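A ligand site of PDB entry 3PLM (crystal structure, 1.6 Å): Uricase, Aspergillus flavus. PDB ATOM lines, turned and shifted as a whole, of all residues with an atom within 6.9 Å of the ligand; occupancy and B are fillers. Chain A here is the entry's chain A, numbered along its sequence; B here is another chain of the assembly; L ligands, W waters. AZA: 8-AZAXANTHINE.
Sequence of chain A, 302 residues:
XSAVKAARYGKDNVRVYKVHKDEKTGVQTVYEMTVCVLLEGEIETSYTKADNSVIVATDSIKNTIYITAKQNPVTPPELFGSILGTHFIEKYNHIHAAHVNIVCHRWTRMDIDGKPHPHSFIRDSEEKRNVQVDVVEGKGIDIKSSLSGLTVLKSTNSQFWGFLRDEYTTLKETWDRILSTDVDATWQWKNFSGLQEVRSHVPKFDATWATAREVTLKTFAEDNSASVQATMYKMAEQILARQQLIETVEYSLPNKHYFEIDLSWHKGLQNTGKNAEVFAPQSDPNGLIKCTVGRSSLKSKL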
ATOM      1  N   SER A 158      25.850  -4.826 -16.179  1.00  0.00           N
ATOM      2  CA  SER A 158      26.054  -5.048 -17.590  1.00  0.00           C
ATOM      3  C   SER A 158      24.667  -5.075 -18.229  1.00  0.00           C
ATOM      4  O   SER A 158      23.740  -5.679 -17.686  1.00  0.00           O
ATOM      5  CB  SER A 158      26.808  -6.366 -17.846  1.00  0.00           C
ATOM      6  OG  SER A 158      26.800  -6.701 -19.230  1.00  0.00           O
ATOM      7  N   GLN A 159      24.551  -4.423 -19.382  1.00  0.00           N
ATOM      8  CA  GLN A 159      23.308  -4.290 -20.122  1.00  0.00           C
ATOM      9  C   GLN A 159      23.581  -4.626 -21.574  1.00  0.00           C
ATOM     10  O   GLN A 159      24.728  -4.530 -22.053  1.00  0.00           O
ATOM     11  CB  GLN A 159      22.802  -2.830 -20.059  1.00  0.00           C
ATOM     12  CG  GLN A 159      22.662  -2.326 -18.644  1.00  0.00           C
ATOM     13  CD  GLN A 159      22.049  -0.924 -18.540  1.00  0.00           C
ATOM     14  OE1 GLN A 159      21.657  -0.318 -19.541  1.00  0.00           O
ATOM     15  NE2 GLN A 159      21.970  -0.425 -17.320  1.00  0.00           N
ATOM     16  N   PHE A 160      22.524  -4.979 -22.279  1.00  0.00           N
ATOM     17  CA  PHE A 160      22.620  -5.095 -23.715  1.00  0.00           C
ATOM     18  C   PHE A 160      21.248  -4.959 -24.342  1.00  0.00           C
ATOM     19  O   PHE A 160      20.465  -5.886 -24.358  1.00  0.00           O
ATOM     20  CB  PHE A 160      23.340  -6.421 -24.137  1.00  0.00           C
ATOM     21  CG  PHE A 160      23.705  -6.445 -25.603  1.00  0.00           C
ATOM     22  CD1 PHE A 160      24.627  -5.535 -26.124  1.00  0.00           C
ATOM     23  CD2 PHE A 160      23.089  -7.345 -26.486  1.00  0.00           C
ATOM     24  CE1 PHE A 160      24.941  -5.530 -27.487  1.00  0.00           C
ATOM     25  CE2 PHE A 160      23.401  -7.347 -27.842  1.00  0.00           C
ATOM     26  CZ  PHE A 160      24.323  -6.438 -28.349  1.00  0.00           C
ATOM     27  N   PHE A 163      20.040  -3.280 -29.887  1.00  0.00           N
ATOM     28  CA  PHE A 163      20.659  -3.879 -31.069  1.00  0.00           C
ATOM     29  C   PHE A 163      19.655  -4.109 -32.208  1.00  0.00           C
ATOM     30  O   PHE A 163      18.431  -4.018 -31.998  1.00  0.00           O
ATOM     31  CB  PHE A 163      21.355  -5.203 -30.685  1.00  0.00           C
ATOM     32  CG  PHE A 163      20.485  -6.128 -29.884  1.00  0.00           C
ATOM     33  CD1 PHE A 163      20.455  -6.053 -28.502  1.00  0.00           C
ATOM     34  CD2 PHE A 163      19.700  -7.086 -30.538  1.00  0.00           C
ATOM     35  CE1 PHE A 163      19.642  -6.916 -27.738  1.00  0.00           C
ATOM     36  CE2 PHE A 163      18.898  -7.951 -29.803  1.00  0.00           C
ATOM     37  CZ  PHE A 163      18.853  -7.851 -28.414  1.00  0.00           C
ATOM     38  N   LEU A 171      17.014 -12.907 -29.523  1.00  0.00           N
ATOM     39  CA  LEU A 171      17.576 -12.423 -28.264  1.00  0.00           C
ATOM     40  C   LEU A 171      16.729 -11.293 -27.656  1.00  0.00           C
ATOM     41  O   LEU A 171      16.415 -10.311 -28.345  1.00  0.00           O
ATOM     42  CB  LEU A 171      18.992 -11.896 -28.510  1.00  0.00           C
ATOM     43  CG  LEU A 171      19.777 -11.388 -27.278  1.00  0.00           C
ATOM     44  CD1 LEU A 171      20.076 -12.551 -26.326  1.00  0.00           C
ATOM     45  CD2 LEU A 171      21.073 -10.711 -27.712  1.00  0.00           C
ATOM     46  N   ARG A 177      22.550  -8.163 -16.718  1.00  0.00           N
ATOM     47  CA  ARG A 177      23.010  -9.529 -17.065  1.00  0.00           C
ATOM     48  C   ARG A 177      24.367  -9.777 -16.442  1.00  0.00           C
ATOM     49  O   ARG A 177      25.032  -8.856 -15.994  1.00  0.00           O
ATOM     50  CB  ARG A 177      23.089  -9.696 -18.588  1.00  0.00           C
ATOM     51  CG  ARG A 177      24.194  -8.867 -19.214  1.00  0.00           C
ATOM     52  CD  ARG A 177      24.249  -9.045 -20.711  1.00  0.00           C
ATOM     53  NE  ARG A 177      25.379  -8.268 -21.265  1.00  0.00           N
ATOM     54  CZ  ARG A 177      25.846  -8.374 -22.508  1.00  0.00           C
ATOM     55  NH1 ARG A 177      25.274  -9.181 -23.415  1.00  0.00           N
ATOM     56  NH2 ARG A 177      26.898  -7.623 -22.862  1.00  0.00           N
ATOM     57  N   LEU A 179      28.268 -10.642 -16.987  1.00  0.00           N
ATOM     58  CA  LEU A 179      29.288 -10.474 -18.018  1.00  0.00           C
ATOM     59  C   LEU A 179      30.552 -11.167 -17.546  1.00  0.00           C
ATOM     60  O   LEU A 179      31.079 -10.892 -16.486  1.00  0.00           O
ATOM     61  CB  LEU A 179      29.516  -8.985 -18.284  1.00  0.00           C
ATOM     62  CG  LEU A 179      30.552  -8.623 -19.359  1.00  0.00           C
ATOM     63  CD1 LEU A 179      30.090  -9.140 -20.712  1.00  0.00           C
ATOM     64  CD2 LEU A 179      30.687  -7.078 -19.388  1.00  0.00           C
ATOM     65  N   SER A 225      28.228  -1.335 -18.153  1.00  0.00           N
ATOM     66  CA  SER A 225      28.584  -1.687 -19.507  1.00  0.00           C
ATOM     67  C   SER A 225      27.386  -1.723 -20.440  1.00  0.00           C
ATOM     68  O   SER A 225      26.400  -2.433 -20.187  1.00  0.00           O
ATOM     69  CB  SER A 225      29.299  -3.059 -19.477  1.00  0.00           C
ATOM     70  OG  SER A 225      29.535  -3.480 -20.792  1.00  0.00           O
ATOM     71  N   ALA A 226      27.497  -1.008 -21.549  1.00  0.00           N
ATOM     72  CA  ALA A 226      26.475  -0.970 -22.575  1.00  0.00           C
ATOM     73  C   ALA A 226      26.616  -2.131 -23.539  1.00  0.00           C
ATOM     74  O   ALA A 226      25.672  -2.449 -24.279  1.00  0.00           O
ATOM     75  CB  ALA A 226      26.551   0.356 -23.351  1.00  0.00           C
ATOM     76  N   SER A 227      27.807  -2.723 -23.544  1.00  0.00           N
ATOM     77  CA  SER A 227      28.128  -3.847 -24.446  1.00  0.00           C
ATOM     78  C   SER A 227      29.589  -4.177 -24.187  1.00  0.00           C
ATOM     79  O   SER A 227      30.322  -3.378 -23.596  1.00  0.00           O
ATOM     80  CB  SER A 227      27.970  -3.506 -25.935  1.00  0.00           C
ATOM     81  OG  SER A 227      28.885  -2.463 -26.319  1.00  0.00           O
ATOM     82  N   VAL A 228      30.044  -5.332 -24.684  1.00  0.00           N
ATOM     83  CA  VAL A 228      31.458  -5.638 -24.576  1.00  0.00           C
ATOM     84  C   VAL A 228      32.248  -4.615 -25.387  1.00  0.00           C
ATOM     85  O   VAL A 228      33.306  -4.137 -24.947  1.00  0.00           O
ATOM     86  CB  VAL A 228      31.701  -7.094 -25.066  1.00  0.00           C
ATOM     87  CG1 VAL A 228      33.200  -7.389 -25.158  1.00  0.00           C
ATOM     88  CG2 VAL A 228      31.019  -8.047 -24.077  1.00  0.00           C
ATOM     89  N   GLN A 229      31.737  -4.309 -26.573  1.00  0.00           N
ATOM     90  CA  GLN A 229      32.357  -3.337 -27.501  1.00  0.00           C
ATOM     91  C   GLN A 229      32.656  -2.018 -26.790  1.00  0.00           C
ATOM     92  O   GLN A 229      33.796  -1.488 -26.847  1.00  0.00           O
ATOM     93  CB  GLN A 229      31.417  -3.066 -28.672  1.00  0.00           C
ATOM     94  CG  GLN A 229      31.316  -4.227 -29.722  1.00  0.00           C
ATOM     95  CD  GLN A 229      30.271  -5.275 -29.396  1.00  0.00           C
ATOM     96  OE1 GLN A 229      29.898  -5.499 -28.234  1.00  0.00           O
ATOM     97  NE2 GLN A 229      29.826  -5.961 -30.448  1.00  0.00           N
ATOM     98  N   ALA A 230      31.645  -1.464 -26.108  1.00  0.00           N
ATOM     99  CA  ALA A 230      31.814  -0.149 -25.482  1.00  0.00           C
ATOM    100  C   ALA A 230      32.813  -0.165 -24.322  1.00  0.00           C
ATOM    101  O   ALA A 230      33.638   0.754 -24.169  1.00  0.00           O
ATOM    102  CB  ALA A 230      30.450   0.378 -25.036  1.00  0.00           C
ATOM    103  N   ASN A 255      32.666 -13.602 -25.104  1.00  0.00           N
ATOM    104  CA  ASN A 255      31.551 -13.278 -24.250  1.00  0.00           C
ATOM    105  C   ASN A 255      31.049 -14.657 -23.771  1.00  0.00           C
ATOM    106  O   ASN A 255      30.466 -15.387 -24.556  1.00  0.00           O
ATOM    107  CB  ASN A 255      30.520 -12.451 -25.044  1.00  0.00           C
ATOM    108  CG  ASN A 255      29.388 -11.928 -24.165  1.00  0.00           C
ATOM    109  OD1 ASN A 255      29.420 -12.071 -22.934  1.00  0.00           O
ATOM    110  ND2 ASN A 255      28.370 -11.319 -24.801  1.00  0.00           N
ATOM    111  N   HIS A 257      28.732 -16.916 -21.954  1.00  0.00           N
ATOM    112  CA  HIS A 257      27.345 -16.693 -21.580  1.00  0.00           C
ATOM    113  C   HIS A 257      26.905 -17.526 -20.396  1.00  0.00           C
ATOM    114  O   HIS A 257      27.250 -18.696 -20.277  1.00  0.00           O
ATOM    115  CB  HIS A 257      26.410 -16.988 -22.766  1.00  0.00           C
ATOM    116  CG  HIS A 257      26.804 -16.286 -24.027  1.00  0.00           C
ATOM    117  ND1 HIS A 257      26.661 -14.920 -24.206  1.00  0.00           N
ATOM    118  CD2 HIS A 257      27.379 -16.754 -25.173  1.00  0.00           C
ATOM    119  CE1 HIS A 257      27.091 -14.591 -25.419  1.00  0.00           C
ATOM    120  NE2 HIS A 257      27.546 -15.677 -26.007  1.00  0.00           N
ATOM    121  N   GLY A 287      30.219 -15.528 -27.842  1.00  0.00           N
ATOM    122  CA  GLY A 287      30.555 -14.319 -28.591  1.00  0.00           C
ATOM    123  C   GLY A 287      32.054 -14.101 -28.634  1.00  0.00           C
ATOM    124  O   GLY A 287      32.777 -14.544 -27.750  1.00  0.00           O
ATOM    125  N   ILE A 289      34.618 -10.808 -29.595  1.00  0.00           N
ATOM    126  CA  ILE A 289      34.579  -9.373 -29.907  1.00  0.00           C
ATOM    127  C   ILE A 289      36.010  -8.865 -29.933  1.00  0.00           C
ATOM    128  O   ILE A 289      36.748  -9.083 -28.972  1.00  0.00           O
ATOM    129  CB  ILE A 289      33.780  -8.555 -28.845  1.00  0.00           C
ATOM    130  CG1 ILE A 289      32.439  -9.257 -28.450  1.00  0.00           C
ATOM    131  CG2 ILE A 289      33.542  -7.109 -29.396  1.00  0.00           C
ATOM    132  CD1 ILE A 289      31.511  -9.543 -29.521  1.00  0.00           C
ATOM    133  N   TYR B   9      33.654  -8.833 -35.011  1.00  0.00           N
ATOM    134  CA  TYR B   9      32.981  -9.438 -33.878  1.00  0.00           C
ATOM    135  C   TYR B   9      32.036 -10.488 -34.438  1.00  0.00           C
ATOM    136  O   TYR B   9      31.644 -10.426 -35.609  1.00  0.00           O
ATOM    137  CB  TYR B   9      32.227  -8.382 -33.026  1.00  0.00           C
ATOM    138  CG  TYR B   9      30.890  -8.088 -33.626  1.00  0.00           C
ATOM    139  CD1 TYR B   9      30.782  -7.358 -34.797  1.00  0.00           C
ATOM    140  CD2 TYR B   9      29.717  -8.645 -33.089  1.00  0.00           C
ATOM    141  CE1 TYR B   9      29.539  -7.150 -35.414  1.00  0.00           C
ATOM    142  CE2 TYR B   9      28.491  -8.449 -33.685  1.00  0.00           C
ATOM    143  CZ  TYR B   9      28.408  -7.702 -34.861  1.00  0.00           C
ATOM    144  OH  TYR B   9      27.190  -7.514 -35.463  1.00  0.00           O
ATOM    145  N   GLY B  10      31.666 -11.467 -33.622  1.00  0.00           N
ATOM    146  CA  GLY B  10      30.744 -12.489 -34.103  1.00  0.00           C
ATOM    147  C   GLY B  10      30.608 -13.615 -33.105  1.00  0.00           C
ATOM    148  O   GLY B  10      30.711 -13.410 -31.917  1.00  0.00           O
ATOM    149  N   LYS B  11      30.385 -14.821 -33.618  1.00  0.00           N
ATOM    150  CA  LYS B  11      30.105 -15.982 -32.758  1.00  0.00           C
ATOM    151  C   LYS B  11      31.113 -17.063 -33.106  1.00  0.00           C
ATOM    152  O   LYS B  11      31.341 -17.350 -34.297  1.00  0.00           O
ATOM    153  CB  LYS B  11      28.687 -16.503 -32.995  1.00  0.00           C
ATOM    154  CG  LYS B  11      28.134 -17.340 -31.817  1.00  0.00           C
ATOM    155  CD  LYS B  11      27.979 -16.485 -30.572  1.00  0.00           C
ATOM    156  CE  LYS B  11      26.665 -16.726 -29.894  1.00  0.00           C
ATOM    157  NZ  LYS B  11      26.431 -15.685 -28.847  1.00  0.00           N
ATOM    158  N   ASN B  52      24.295   0.636 -30.118  1.00  0.00           N
ATOM    159  CA  ASN B  52      24.066  -0.779 -30.452  1.00  0.00           C
ATOM    160  C   ASN B  52      23.235  -0.999 -31.721  1.00  0.00           C
ATOM    161  O   ASN B  52      23.066  -2.133 -32.158  1.00  0.00           O
ATOM    162  CB  ASN B  52      23.495  -1.554 -29.246  1.00  0.00           C
ATOM    163  CG  ASN B  52      24.489  -1.684 -28.103  1.00  0.00           C
ATOM    164  OD1 ASN B  52      25.705  -1.629 -28.324  1.00  0.00           O
ATOM    165  ND2 ASN B  52      24.000  -1.863 -26.884  1.00  0.00           N
ATOM    166  N   ILE B  55      24.692  -3.176 -34.408  1.00  0.00           N
ATOM    167  CA  ILE B  55      25.103  -4.543 -34.064  1.00  0.00           C
ATOM    168  C   ILE B  55      24.055  -5.592 -34.432  1.00  0.00           C
ATOM    169  O   ILE B  55      22.927  -5.555 -33.941  1.00  0.00           O
ATOM    170  CB  ILE B  55      25.407  -4.686 -32.560  1.00  0.00           C
ATOM    171  CG1 ILE B  55      26.573  -3.781 -32.131  1.00  0.00           C
ATOM    172  CG2 ILE B  55      25.780  -6.182 -32.228  1.00  0.00           C
ATOM    173  CD1 ILE B  55      26.725  -3.724 -30.597  1.00  0.00           C
ATOM    174  N   VAL B  56      24.438  -6.490 -35.346  1.00  0.00           N
ATOM    175  CA  VAL B  56      23.719  -7.727 -35.578  1.00  0.00           C
ATOM    176  C   VAL B  56      24.153  -8.604 -34.390  1.00  0.00           C
ATOM    177  O   VAL B  56      25.340  -8.910 -34.275  1.00  0.00           O
ATOM    178  CB  VAL B  56      24.132  -8.331 -36.943  1.00  0.00           C
ATOM    179  CG1 VAL B  56      23.482  -9.715 -37.147  1.00  0.00           C
ATOM    180  CG2 VAL B  56      23.726  -7.368 -38.077  1.00  0.00           C
ATOM    181  N   ALA B  57      23.224  -8.946 -33.486  1.00  0.00           N
ATOM    182  CA  ALA B  57      23.627  -9.623 -32.231  1.00  0.00           C
ATOM    183  C   ALA B  57      24.321 -10.947 -32.555  1.00  0.00           C
ATOM    184  O   ALA B  57      23.966 -11.620 -33.509  1.00  0.00           O
ATOM    185  CB  ALA B  57      22.427  -9.835 -31.283  1.00  0.00           C
ATOM    186  N   THR B  58      25.326 -11.298 -31.744  1.00  0.00           N
ATOM    187  CA  THR B  58      26.066 -12.535 -31.992  1.00  0.00           C
ATOM    188  C   THR B  58      25.098 -13.701 -31.869  1.00  0.00           C
ATOM    189  O   THR B  58      25.225 -14.686 -32.610  1.00  0.00           O
ATOM    190  CB  THR B  58      27.274 -12.726 -31.043  1.00  0.00           C
ATOM    191  OG1 THR B  58      26.807 -12.914 -29.709  1.00  0.00           O
ATOM    192  CG2 THR B  58      28.190 -11.513 -31.146  1.00  0.00           C
ATOM    193  N   ASP B  59      24.099 -13.585 -30.979  1.00  0.00           N
ATOM    194  CA  ASP B  59      23.044 -14.593 -30.879  1.00  0.00           C
ATOM    195  C   ASP B  59      22.305 -14.788 -32.213  1.00  0.00           C
ATOM    196  O   ASP B  59      21.972 -15.903 -32.588  1.00  0.00           O
ATOM    197  CB  ASP B  59      22.047 -14.233 -29.776  1.00  0.00           C
ATOM    198  CG  ASP B  59      21.102 -15.382 -29.468  1.00  0.00           C
ATOM    199  OD1 ASP B  59      21.546 -16.342 -28.792  1.00  0.00           O
ATOM    200  OD2 ASP B  59      19.939 -15.322 -29.907  1.00  0.00           O
ATOM    201  N   SER B  60      22.041 -13.678 -32.930  1.00  0.00           N
ATOM    202  CA  SER B  60      21.411 -13.753 -34.254  1.00  0.00           C
ATOM    203  C   SER B  60      22.320 -14.401 -35.299  1.00  0.00           C
ATOM    204  O   SER B  60      21.847 -15.085 -36.210  1.00  0.00           O
ATOM    205  CB  SER B  60      20.964 -12.351 -34.721  1.00  0.00           C
ATOM    206  OG  SER B  60      20.213 -11.775 -33.675  1.00  0.00           O
HETATM  207  N1  AZA L   1      27.903  -7.586 -27.618  1.00  0.00           N
HETATM  208  C2  AZA L   1      27.499  -7.880 -26.361  1.00  0.00           C
HETATM  209  O2  AZA L   1      28.037  -7.268 -25.433  1.00  0.00           O
HETATM  210  N3  AZA L   1      26.538  -8.830 -26.055  1.00  0.00           N
HETATM  211  C4  AZA L   1      25.940  -9.460 -27.080  1.00  0.00           C
HETATM  212  C5  AZA L   1      26.339  -9.175 -28.465  1.00  0.00           C
HETATM  213  C6  AZA L   1      27.375  -8.150 -28.700  1.00  0.00           C
HETATM  214  O6  AZA L   1      27.761  -7.908 -29.854  1.00  0.00           O
HETATM  215  N7  AZA L   1      25.603  -9.920 -29.310  1.00  0.00           N
HETATM  216  N8  AZA L   1      24.781 -10.681 -28.530  1.00  0.00           N
HETATM  217  N9  AZA L   1      24.982 -10.409 -27.185  1.00  0.00           N
HETATM  218  O   HOH W   1      23.994 -11.859 -25.108  1.00  0.00           O
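The backbone NH (N) of Val 228 lies within hydrogen-bond range of an oxygen (O2) of the ligand, at 2.9 Å.
NE2 of Gln 229 is in hydrogen-bond range of O6 of the ligand.
The guanidinium group of Arg 177 sits at hydrogen-bond distance from an oxygen (O2) of the ligand, at 2.8 Å.
The side-chain amide nitrogen (ND2) of Asn 255 sits close to a nitrogen (N3) of the ligand (3.3 Å).
The side-chain hydroxyl (OG1) of Thr 58 of chain B sits at hydrogen-bond distance from a nitrogen (N8) of the ligand (3.2 Å).
N7 of the ligand sits at hydrogen-bond distance from N of Thr 58 of chain B, 2.8 Å away.
NE2 of His 257 is in hydrogen-bond range of O of Asn 255, at 3.3 Å.
The backbone NH of Arg 177 is in hydrogen-bond range of the backbone carbonyl oxygen of Ser 158 (2.9 Å).
N of Asn 255 lies within hydrogen-bond range of O of Gly 287, at 2.8 Å.
The side-chain hydroxyl of Ser 227 lies within hydrogen-bond range of the backbone NH of Ala 230 (2.9 Å).
The side-chain hydroxyl (OG) of Ser 227 lies close to the backbone NH (N) of Gln 229 (3.4 Å).
The side-chain hydroxyl (OH) of Tyr 9 of chain B lies within hydrogen-bond range of the backbone carbonyl oxygen (O) of Val 56 of chain B, 2.6 Å away.
The side-chain hydroxyl of Ser 225 lies within hydrogen-bond range of the backbone carbonyl oxygen of Ser 227 (2.9 Å).
The side-chain hydroxyl (OG1) of Thr 58 of chain B lies within hydrogen-bond range of the side-chain amino group (NZ) of Lys 11 of chain B (2.9 Å).
Residues that only touch the ligand: Phe 160, Ala 57 of chain B, Ile 55 of chain B, Ser 227, Leu 171, Tyr 9 of chain B and Asp 59 of chain B.
Water W1 lies within hydrogen-bond range of N9 of the ligand (2.7 Å) and NH1 of Arg 177 (3.4 Å).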
